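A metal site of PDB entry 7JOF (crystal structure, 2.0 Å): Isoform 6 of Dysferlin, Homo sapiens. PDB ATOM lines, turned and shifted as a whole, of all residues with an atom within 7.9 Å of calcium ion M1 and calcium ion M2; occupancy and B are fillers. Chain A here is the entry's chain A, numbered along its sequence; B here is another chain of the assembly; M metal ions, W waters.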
ATOM      1  N   THR A  20       3.202  -5.793 -10.333  1.00  0.00           N
ATOM      2  CA  THR A  20       4.186  -6.809  -9.883  1.00  0.00           C
ATOM      3  C   THR A  20       5.301  -6.142  -9.087  1.00  0.00           C
ATOM      4  O   THR A  20       5.441  -4.925  -9.119  1.00  0.00           O
ATOM      5  CB  THR A  20       4.907  -7.524 -11.032  1.00  0.00           C
ATOM      6  OG1 THR A  20       5.901  -6.713 -11.647  1.00  0.00           O
ATOM      7  CG2 THR A  20       3.961  -8.023 -12.082  1.00  0.00           C
ATOM      8  N   ASP A  22       8.370  -5.736  -9.932  1.00  0.00           N
ATOM      9  CA  ASP A  22       9.526  -5.211 -10.718  1.00  0.00           C
ATOM     10  C   ASP A  22       9.039  -4.620 -12.045  1.00  0.00           C
ATOM     11  O   ASP A  22       7.916  -4.240 -12.125  1.00  0.00           O
ATOM     12  CB  ASP A  22      10.629  -6.245 -10.944  1.00  0.00           C
ATOM     13  CG  ASP A  22      10.097  -7.580 -11.417  1.00  0.00           C
ATOM     14  OD1 ASP A  22       9.105  -7.577 -12.082  1.00  0.00           O
ATOM     15  OD2 ASP A  22      10.696  -8.558 -11.084  1.00  0.00           O
ATOM     16  N   THR A  23       9.890  -4.650 -13.077  1.00  0.00           N
ATOM     17  CA  THR A  23       9.608  -4.071 -14.421  1.00  0.00           C
ATOM     18  C   THR A  23       8.605  -4.920 -15.227  1.00  0.00           C
ATOM     19  O   THR A  23       8.075  -4.410 -16.185  1.00  0.00           O
ATOM     20  CB  THR A  23      10.907  -3.798 -15.180  1.00  0.00           C
ATOM     21  OG1 THR A  23      11.494  -5.077 -15.407  1.00  0.00           O
ATOM     22  CG2 THR A  23      11.842  -2.837 -14.456  1.00  0.00           C
ATOM     23  N   ASP A  24       8.393  -6.170 -14.819  1.00  0.00           N
ATOM     24  CA  ASP A  24       7.450  -7.099 -15.504  1.00  0.00           C
ATOM     25  C   ASP A  24       6.027  -6.558 -15.382  1.00  0.00           C
ATOM     26  O   ASP A  24       5.672  -6.060 -14.287  1.00  0.00           O
ATOM     27  CB  ASP A  24       7.576  -8.518 -14.968  1.00  0.00           C
ATOM     28  CG  ASP A  24       6.522  -9.461 -15.518  1.00  0.00           C
ATOM     29  OD1 ASP A  24       6.411  -9.555 -16.759  1.00  0.00           O
ATOM     30  OD2 ASP A  24       5.823 -10.101 -14.703  1.00  0.00           O
ATOM     31  N   ILE A  25       5.245  -6.649 -16.460  1.00  0.00           N
ATOM     32  CA  ILE A  25       3.837  -6.170 -16.481  1.00  0.00           C
ATOM     33  C   ILE A  25       3.023  -7.356 -15.973  1.00  0.00           C
ATOM     34  O   ILE A  25       3.166  -8.381 -16.549  1.00  0.00           O
ATOM     35  CB  ILE A  25       3.439  -5.745 -17.896  1.00  0.00           C
ATOM     36  CG1 ILE A  25       4.390  -4.681 -18.476  1.00  0.00           C
ATOM     37  CG2 ILE A  25       2.003  -5.276 -17.913  1.00  0.00           C
ATOM     38  CD1 ILE A  25       4.796  -3.643 -17.500  1.00  0.00           C
ATOM     39  N   SER A  26       2.260  -7.185 -14.893  1.00  0.00           N
ATOM     40  CA  SER A  26       1.422  -8.253 -14.264  1.00  0.00           C
ATOM     41  C   SER A  26       0.840  -9.291 -15.249  1.00  0.00           C
ATOM     42  O   SER A  26       0.208  -8.924 -16.237  1.00  0.00           O
ATOM     43  CB  SER A  26       0.347  -7.661 -13.371  1.00  0.00           C
ATOM     44  OG  SER A  26       0.889  -6.893 -12.318  1.00  0.00           O
ATOM     45  N   ASP A  27       1.072 -10.552 -14.938  1.00  0.00           N
ATOM     46  CA  ASP A  27       0.468 -11.702 -15.658  1.00  0.00           C
ATOM     47  C   ASP A  27      -0.464 -12.301 -14.618  1.00  0.00           C
ATOM     48  O   ASP A  27      -0.136 -13.307 -13.993  1.00  0.00           O
ATOM     49  CB  ASP A  27       1.522 -12.646 -16.185  1.00  0.00           C
ATOM     50  CG  ASP A  27       2.580 -11.916 -16.959  1.00  0.00           C
ATOM     51  OD1 ASP A  27       2.254 -11.373 -18.021  1.00  0.00           O
ATOM     52  OD2 ASP A  27       3.668 -11.874 -16.475  1.00  0.00           O
ATOM     53  N   ALA A  28      -1.558 -11.582 -14.436  1.00  0.00           N
ATOM     54  CA  ALA A  28      -2.442 -11.848 -13.298  1.00  0.00           C
ATOM     55  C   ALA A  28      -3.466 -12.935 -13.543  1.00  0.00           C
ATOM     56  O   ALA A  28      -3.986 -13.061 -14.642  1.00  0.00           O
ATOM     57  CB  ALA A  28      -3.110 -10.580 -12.826  1.00  0.00           C
ATOM     58  N   VAL A  43      -4.624 -16.850 -16.998  1.00  0.00           N
ATOM     59  CA  VAL A  43      -3.621 -15.770 -16.853  1.00  0.00           C
ATOM     60  C   VAL A  43      -3.879 -14.697 -17.919  1.00  0.00           C
ATOM     61  O   VAL A  43      -4.038 -15.050 -19.090  1.00  0.00           O
ATOM     62  CB  VAL A  43      -2.198 -16.355 -17.016  1.00  0.00           C
ATOM     63  CG1 VAL A  43      -1.104 -15.328 -17.090  1.00  0.00           C
ATOM     64  CG2 VAL A  43      -1.864 -17.402 -15.972  1.00  0.00           C
ATOM     65  N   ILE A  44      -4.045 -13.453 -17.505  1.00  0.00           N
ATOM     66  CA  ILE A  44      -4.133 -12.358 -18.518  1.00  0.00           C
ATOM     67  C   ILE A  44      -2.692 -11.869 -18.719  1.00  0.00           C
ATOM     68  O   ILE A  44      -2.162 -11.261 -17.821  1.00  0.00           O
ATOM     69  CB  ILE A  44      -5.067 -11.205 -18.098  1.00  0.00           C
ATOM     70  CG1 ILE A  44      -6.531 -11.640 -17.965  1.00  0.00           C
ATOM     71  CG2 ILE A  44      -4.880 -10.062 -19.079  1.00  0.00           C
ATOM     72  CD1 ILE A  44      -6.943 -12.705 -18.904  1.00  0.00           C
ATOM     73  N   LYS A  45      -2.096 -12.161 -19.847  1.00  0.00           N
ATOM     74  CA  LYS A  45      -0.690 -11.738 -20.086  1.00  0.00           C
ATOM     75  C   LYS A  45      -0.567 -10.207 -20.162  1.00  0.00           C
ATOM     76  O   LYS A  45      -1.393  -9.574 -20.818  1.00  0.00           O
ATOM     77  CB  LYS A  45      -0.158 -12.320 -21.400  1.00  0.00           C
ATOM     78  CG  LYS A  45      -0.601 -13.740 -21.717  1.00  0.00           C
ATOM     79  CD  LYS A  45      -0.130 -14.210 -23.072  1.00  0.00           C
ATOM     80  CE  LYS A  45      -0.529 -15.640 -23.369  1.00  0.00           C
ATOM     81  NZ  LYS A  45       0.635 -16.443 -23.826  1.00  0.00           N
ATOM     82  N   ASN A  46       0.444  -9.668 -19.498  1.00  0.00           N
ATOM     83  CA  ASN A  46       0.846  -8.240 -19.639  1.00  0.00           C
ATOM     84  C   ASN A  46      -0.314  -7.235 -19.446  1.00  0.00           C
ATOM     85  O   ASN A  46      -0.581  -6.493 -20.364  1.00  0.00           O
ATOM     86  CB  ASN A  46       1.509  -8.059 -21.012  1.00  0.00           C
ATOM     87  CG  ASN A  46       2.832  -8.788 -21.077  1.00  0.00           C
ATOM     88  OD1 ASN A  46       3.524  -8.797 -20.098  1.00  0.00           O
ATOM     89  ND2 ASN A  46       3.203  -9.356 -22.199  1.00  0.00           N
ATOM     90  N   SER A  47      -0.950  -7.248 -18.294  1.00  0.00           N
ATOM     91  CA  SER A  47      -1.974  -6.244 -17.981  1.00  0.00           C
ATOM     92  C   SER A  47      -2.022  -5.916 -16.495  1.00  0.00           C
ATOM     93  O   SER A  47      -2.205  -6.795 -15.698  1.00  0.00           O
ATOM     94  CB  SER A  47      -3.329  -6.566 -18.551  1.00  0.00           C
ATOM     95  OG  SER A  47      -4.300  -5.791 -17.944  1.00  0.00           O
ATOM     96  N   LYS A  76      -2.256 -13.774  -8.089  1.00  0.00           N
ATOM     97  CA  LYS A  76      -0.833 -14.117  -8.305  1.00  0.00           C
ATOM     98  C   LYS A  76      -0.333 -13.676  -9.687  1.00  0.00           C
ATOM     99  O   LYS A  76      -1.140 -13.560 -10.625  1.00  0.00           O
ATOM    100  CB  LYS A  76      -0.588 -15.605  -8.107  1.00  0.00           C
ATOM    101  CG  LYS A  76      -0.797 -16.090  -6.679  1.00  0.00           C
ATOM    102  CD  LYS A  76      -0.146 -17.373  -6.331  1.00  0.00           C
ATOM    103  CE  LYS A  76      -1.071 -18.558  -6.182  1.00  0.00           C
ATOM    104  NZ  LYS A  76      -0.323 -19.828  -6.032  1.00  0.00           N
ATOM    105  N   ASP A  77       0.968 -13.465  -9.784  1.00  0.00           N
ATOM    106  CA  ASP A  77       1.614 -13.109 -11.057  1.00  0.00           C
ATOM    107  C   ASP A  77       2.274 -14.357 -11.643  1.00  0.00           C
ATOM    108  O   ASP A  77       3.209 -14.863 -11.052  1.00  0.00           O
ATOM    109  CB  ASP A  77       2.586 -11.952 -10.936  1.00  0.00           C
ATOM    110  CG  ASP A  77       3.474 -11.896 -12.173  1.00  0.00           C
ATOM    111  OD1 ASP A  77       2.940 -11.753 -13.275  1.00  0.00           O
ATOM    112  OD2 ASP A  77       4.677 -12.048 -11.987  1.00  0.00           O
ATOM    113  N   HIS A  78       1.715 -14.826 -12.748  1.00  0.00           N
ATOM    114  CA  HIS A  78       2.284 -15.969 -13.516  1.00  0.00           C
ATOM    115  C   HIS A  78       3.787 -15.707 -13.790  1.00  0.00           C
ATOM    116  O   HIS A  78       4.082 -14.682 -14.312  1.00  0.00           O
ATOM    117  CB  HIS A  78       1.565 -16.125 -14.855  1.00  0.00           C
ATOM    118  CG  HIS A  78       2.175 -17.222 -15.646  1.00  0.00           C
ATOM    119  ND1 HIS A  78       3.104 -17.004 -16.617  1.00  0.00           N
ATOM    120  CD2 HIS A  78       2.060 -18.559 -15.544  1.00  0.00           C
ATOM    121  CE1 HIS A  78       3.465 -18.164 -17.121  1.00  0.00           C
ATOM    122  NE2 HIS A  78       2.850 -19.110 -16.490  1.00  0.00           N
ATOM    123  N   GLU A  79       4.661 -16.647 -13.468  1.00  0.00           N
ATOM    124  CA  GLU A  79       6.099 -16.359 -13.732  1.00  0.00           C
ATOM    125  C   GLU A  79       6.607 -17.250 -14.878  1.00  0.00           C
ATOM    126  O   GLU A  79       6.709 -18.434 -14.671  1.00  0.00           O
ATOM    127  CB  GLU A  79       6.806 -16.497 -12.393  1.00  0.00           C
ATOM    128  CG  GLU A  79       8.145 -15.823 -12.340  1.00  0.00           C
ATOM    129  CD  GLU A  79       8.196 -14.338 -12.630  1.00  0.00           C
ATOM    130  OE1 GLU A  79       7.156 -13.734 -12.914  1.00  0.00           O
ATOM    131  OE2 GLU A  79       9.278 -13.821 -12.600  1.00  0.00           O
ATOM    132  N   THR A  80       6.950 -16.648 -16.025  1.00  0.00           N
ATOM    133  CA  THR A  80       7.356 -17.293 -17.322  1.00  0.00           C
ATOM    134  C   THR A  80       8.224 -18.528 -17.070  1.00  0.00           C
ATOM    135  O   THR A  80       9.472 -18.387 -17.036  1.00  0.00           O
ATOM    136  CB  THR A  80       7.957 -16.276 -18.316  1.00  0.00           C
ATOM    137  OG1 THR A  80       7.874 -14.948 -17.833  1.00  0.00           O
ATOM    138  CG2 THR A  80       7.361 -16.331 -19.707  1.00  0.00           C
ATOM    139  N   MET A  81       7.532 -19.657 -16.830  1.00  0.00           N
ATOM    140  CA  MET A  81       8.036 -21.004 -16.506  1.00  0.00           C
ATOM    141  C   MET A  81       8.676 -21.014 -15.113  1.00  0.00           C
ATOM    142  O   MET A  81       9.921 -20.969 -15.005  1.00  0.00           O
ATOM    143  CB  MET A  81       9.000 -21.512 -17.577  1.00  0.00           C
ATOM    144  CG  MET A  81       8.503 -22.732 -18.333  1.00  0.00           C
ATOM    145  SD  MET A  81       9.739 -24.056 -18.257  1.00  0.00           S
ATOM    146  CE  MET A  81      10.983 -23.315 -17.195  1.00  0.00           C
ATOM    147  N   ARG A  83       7.622 -20.737 -10.435  1.00  0.00           N
ATOM    148  CA  ARG A  83       6.697 -20.542  -9.296  1.00  0.00           C
ATOM    149  C   ARG A  83       6.165 -19.117  -9.358  1.00  0.00           C
ATOM    150  O   ARG A  83       6.936 -18.165  -9.379  1.00  0.00           O
ATOM    151  CB  ARG A  83       7.356 -20.974  -7.980  1.00  0.00           C
ATOM    152  CG  ARG A  83       6.416 -20.998  -6.784  1.00  0.00           C
ATOM    153  CD  ARG A  83       6.181 -22.408  -6.293  1.00  0.00           C
ATOM    154  NE  ARG A  83       5.684 -22.476  -4.930  1.00  0.00           N
ATOM    155  CZ  ARG A  83       6.356 -22.997  -3.918  1.00  0.00           C
ATOM    156  NH1 ARG A  83       5.849 -24.008  -3.245  1.00  0.00           N
ATOM    157  NH2 ARG A  83       7.548 -22.523  -3.586  1.00  0.00           N
ATOM    158  N   ASN A  84       4.839 -19.020  -9.405  1.00  0.00           N
ATOM    159  CA  ASN A  84       4.092 -17.742  -9.495  1.00  0.00           C
ATOM    160  C   ASN A  84       4.324 -16.931  -8.227  1.00  0.00           C
ATOM    161  O   ASN A  84       4.525 -17.534  -7.165  1.00  0.00           O
ATOM    162  CB  ASN A  84       2.666 -18.041  -9.950  1.00  0.00           C
ATOM    163  CG  ASN A  84       2.698 -19.092 -11.046  1.00  0.00           C
ATOM    164  OD1 ASN A  84       3.594 -19.107 -11.879  1.00  0.00           O
ATOM    165  ND2 ASN A  84       1.668 -19.910 -11.096  1.00  0.00           N
ATOM    166  N   ARG A  85       4.241 -15.609  -8.322  1.00  0.00           N
ATOM    167  CA  ARG A  85       4.476 -14.711  -7.170  1.00  0.00           C
ATOM    168  C   ARG A  85       3.182 -14.041  -6.700  1.00  0.00           C
ATOM    169  O   ARG A  85       2.374 -13.618  -7.503  1.00  0.00           O
ATOM    170  CB  ARG A  85       5.603 -13.713  -7.476  1.00  0.00           C
ATOM    171  CG  ARG A  85       5.671 -13.294  -8.935  1.00  0.00           C
ATOM    172  CD  ARG A  85       6.963 -12.652  -9.374  1.00  0.00           C
ATOM    173  NE  ARG A  85       6.741 -11.494 -10.190  1.00  0.00           N
ATOM    174  CZ  ARG A  85       7.702 -10.703 -10.644  1.00  0.00           C
ATOM    175  NH1 ARG A  85       8.668 -10.261  -9.858  1.00  0.00           N
ATOM    176  NH2 ARG A  85       7.648 -10.340 -11.899  1.00  0.00           N
ATOM    177  N   LEU A  87       0.629 -11.399  -5.400  1.00  0.00           N
ATOM    178  CA  LEU A  87       0.441  -9.967  -5.712  1.00  0.00           C
ATOM    179  C   LEU A  87      -0.456  -9.351  -4.632  1.00  0.00           C
ATOM    180  O   LEU A  87      -0.176  -8.336  -4.193  1.00  0.00           O
ATOM    181  CB  LEU A  87      -0.162  -9.799  -7.107  1.00  0.00           C
ATOM    182  CG  LEU A  87       0.744 -10.072  -8.308  1.00  0.00           C
ATOM    183  CD1 LEU A  87       0.125  -9.553  -9.590  1.00  0.00           C
ATOM    184  CD2 LEU A  87       2.139  -9.539  -8.094  1.00  0.00           C
ATOM    185  N   THR B 114      13.594  -9.896 -12.262  1.00  0.00           N
ATOM    186  CA  THR B 114      13.225 -11.121 -13.014  1.00  0.00           C
ATOM    187  C   THR B 114      13.312 -10.860 -14.519  1.00  0.00           C
ATOM    188  O   THR B 114      13.339 -11.847 -15.274  1.00  0.00           O
ATOM    189  CB  THR B 114      11.822 -11.608 -12.615  1.00  0.00           C
ATOM    190  OG1 THR B 114      10.903 -10.540 -12.860  1.00  0.00           O
ATOM    191  CG2 THR B 114      11.733 -12.046 -11.171  1.00  0.00           C
ATOM    192  N   LYS B 115      13.332  -9.593 -14.944  1.00  0.00           N
ATOM    193  CA  LYS B 115      13.367  -9.231 -16.381  1.00  0.00           C
ATOM    194  C   LYS B 115      14.740  -8.673 -16.769  1.00  0.00           C
ATOM    195  O   LYS B 115      14.857  -8.085 -17.861  1.00  0.00           O
ATOM    196  CB  LYS B 115      12.251  -8.239 -16.715  1.00  0.00           C
ATOM    197  CG  LYS B 115      10.853  -8.821 -16.784  1.00  0.00           C
ATOM    198  CD  LYS B 115      10.670  -9.807 -17.914  1.00  0.00           C
ATOM    199  CE  LYS B 115       9.213 -10.154 -18.177  1.00  0.00           C
ATOM    200  NZ  LYS B 115       8.870 -11.494 -17.651  1.00  0.00           N
HETATM  201 CA    CA M   1       4.582  -9.985 -18.071  1.00  0.00          CA
HETATM  202 CA    CA M   2       5.206 -12.591 -14.531  1.00  0.00          CA
HETATM  203  O   HOH W   1       6.316 -11.649 -19.164  1.00  0.00           O
HETATM  204  O   HOH W   2       5.995  -7.908 -18.967  1.00  0.00           O
HETATM  205  O   HOH W   3       6.745 -13.036 -16.454  1.00  0.00           O
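The backbone NH (N) of Asp 77 is in hydrogen-bond range of the backbone carbonyl oxygen (O) of Arg 85. NZ of Lys 115 of chain B sits close to OD1 of Asp 24, at 3.3 Å. The backbone NH (N) of Asp 24 is in hydrogen-bond range of the side-chain carboxylate (OD1) of Asp 22 (3.2 Å). OD1 of Asn 84 sits at hydrogen-bond distance from N of Glu 79 (3.1 Å). The guanidinium group (NH2) of Arg 85 lies within salt-bridge range of the side-chain carboxylate (OE2) of Glu 79 (3.9 Å). OD2 of Asp 24 sits close to NH2 of Arg 85. The backbone carbonyl oxygen (O) of Ser 26 is in hydrogen-bond range of the backbone NH (N) of Asn 46. The side-chain hydroxyl (OG1) of Thr 20 is in hydrogen-bond range of the backbone carbonyl oxygen (O) of Asp 24, 2.7 Å away.
Calcium ion M2 is bound by O of His 78, water W3, OD2 of Asp 24, OD2 of Asp 27, OD2 of Asp 77, OD1 of Asp 77 and OE1 of Glu 79.
Calcium ion M1 is bound by OD1 of Asp 24 (2.3 Å), OD1 of Asn 46 (2.6 Å), O of Ile 25 (2.6 Å), OD2 of Asp 27 (2.6 Å), water W1 (2.6 Å), water W2 (2.7 Å) and OD1 of Asp 27 (2.7 Å).
Water W3 bridges OG1 of Thr 80 and NZ of Lys 115 of chain B.
Of the 25 residues printed, 5 come within 4 Å of calcium ion M2.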
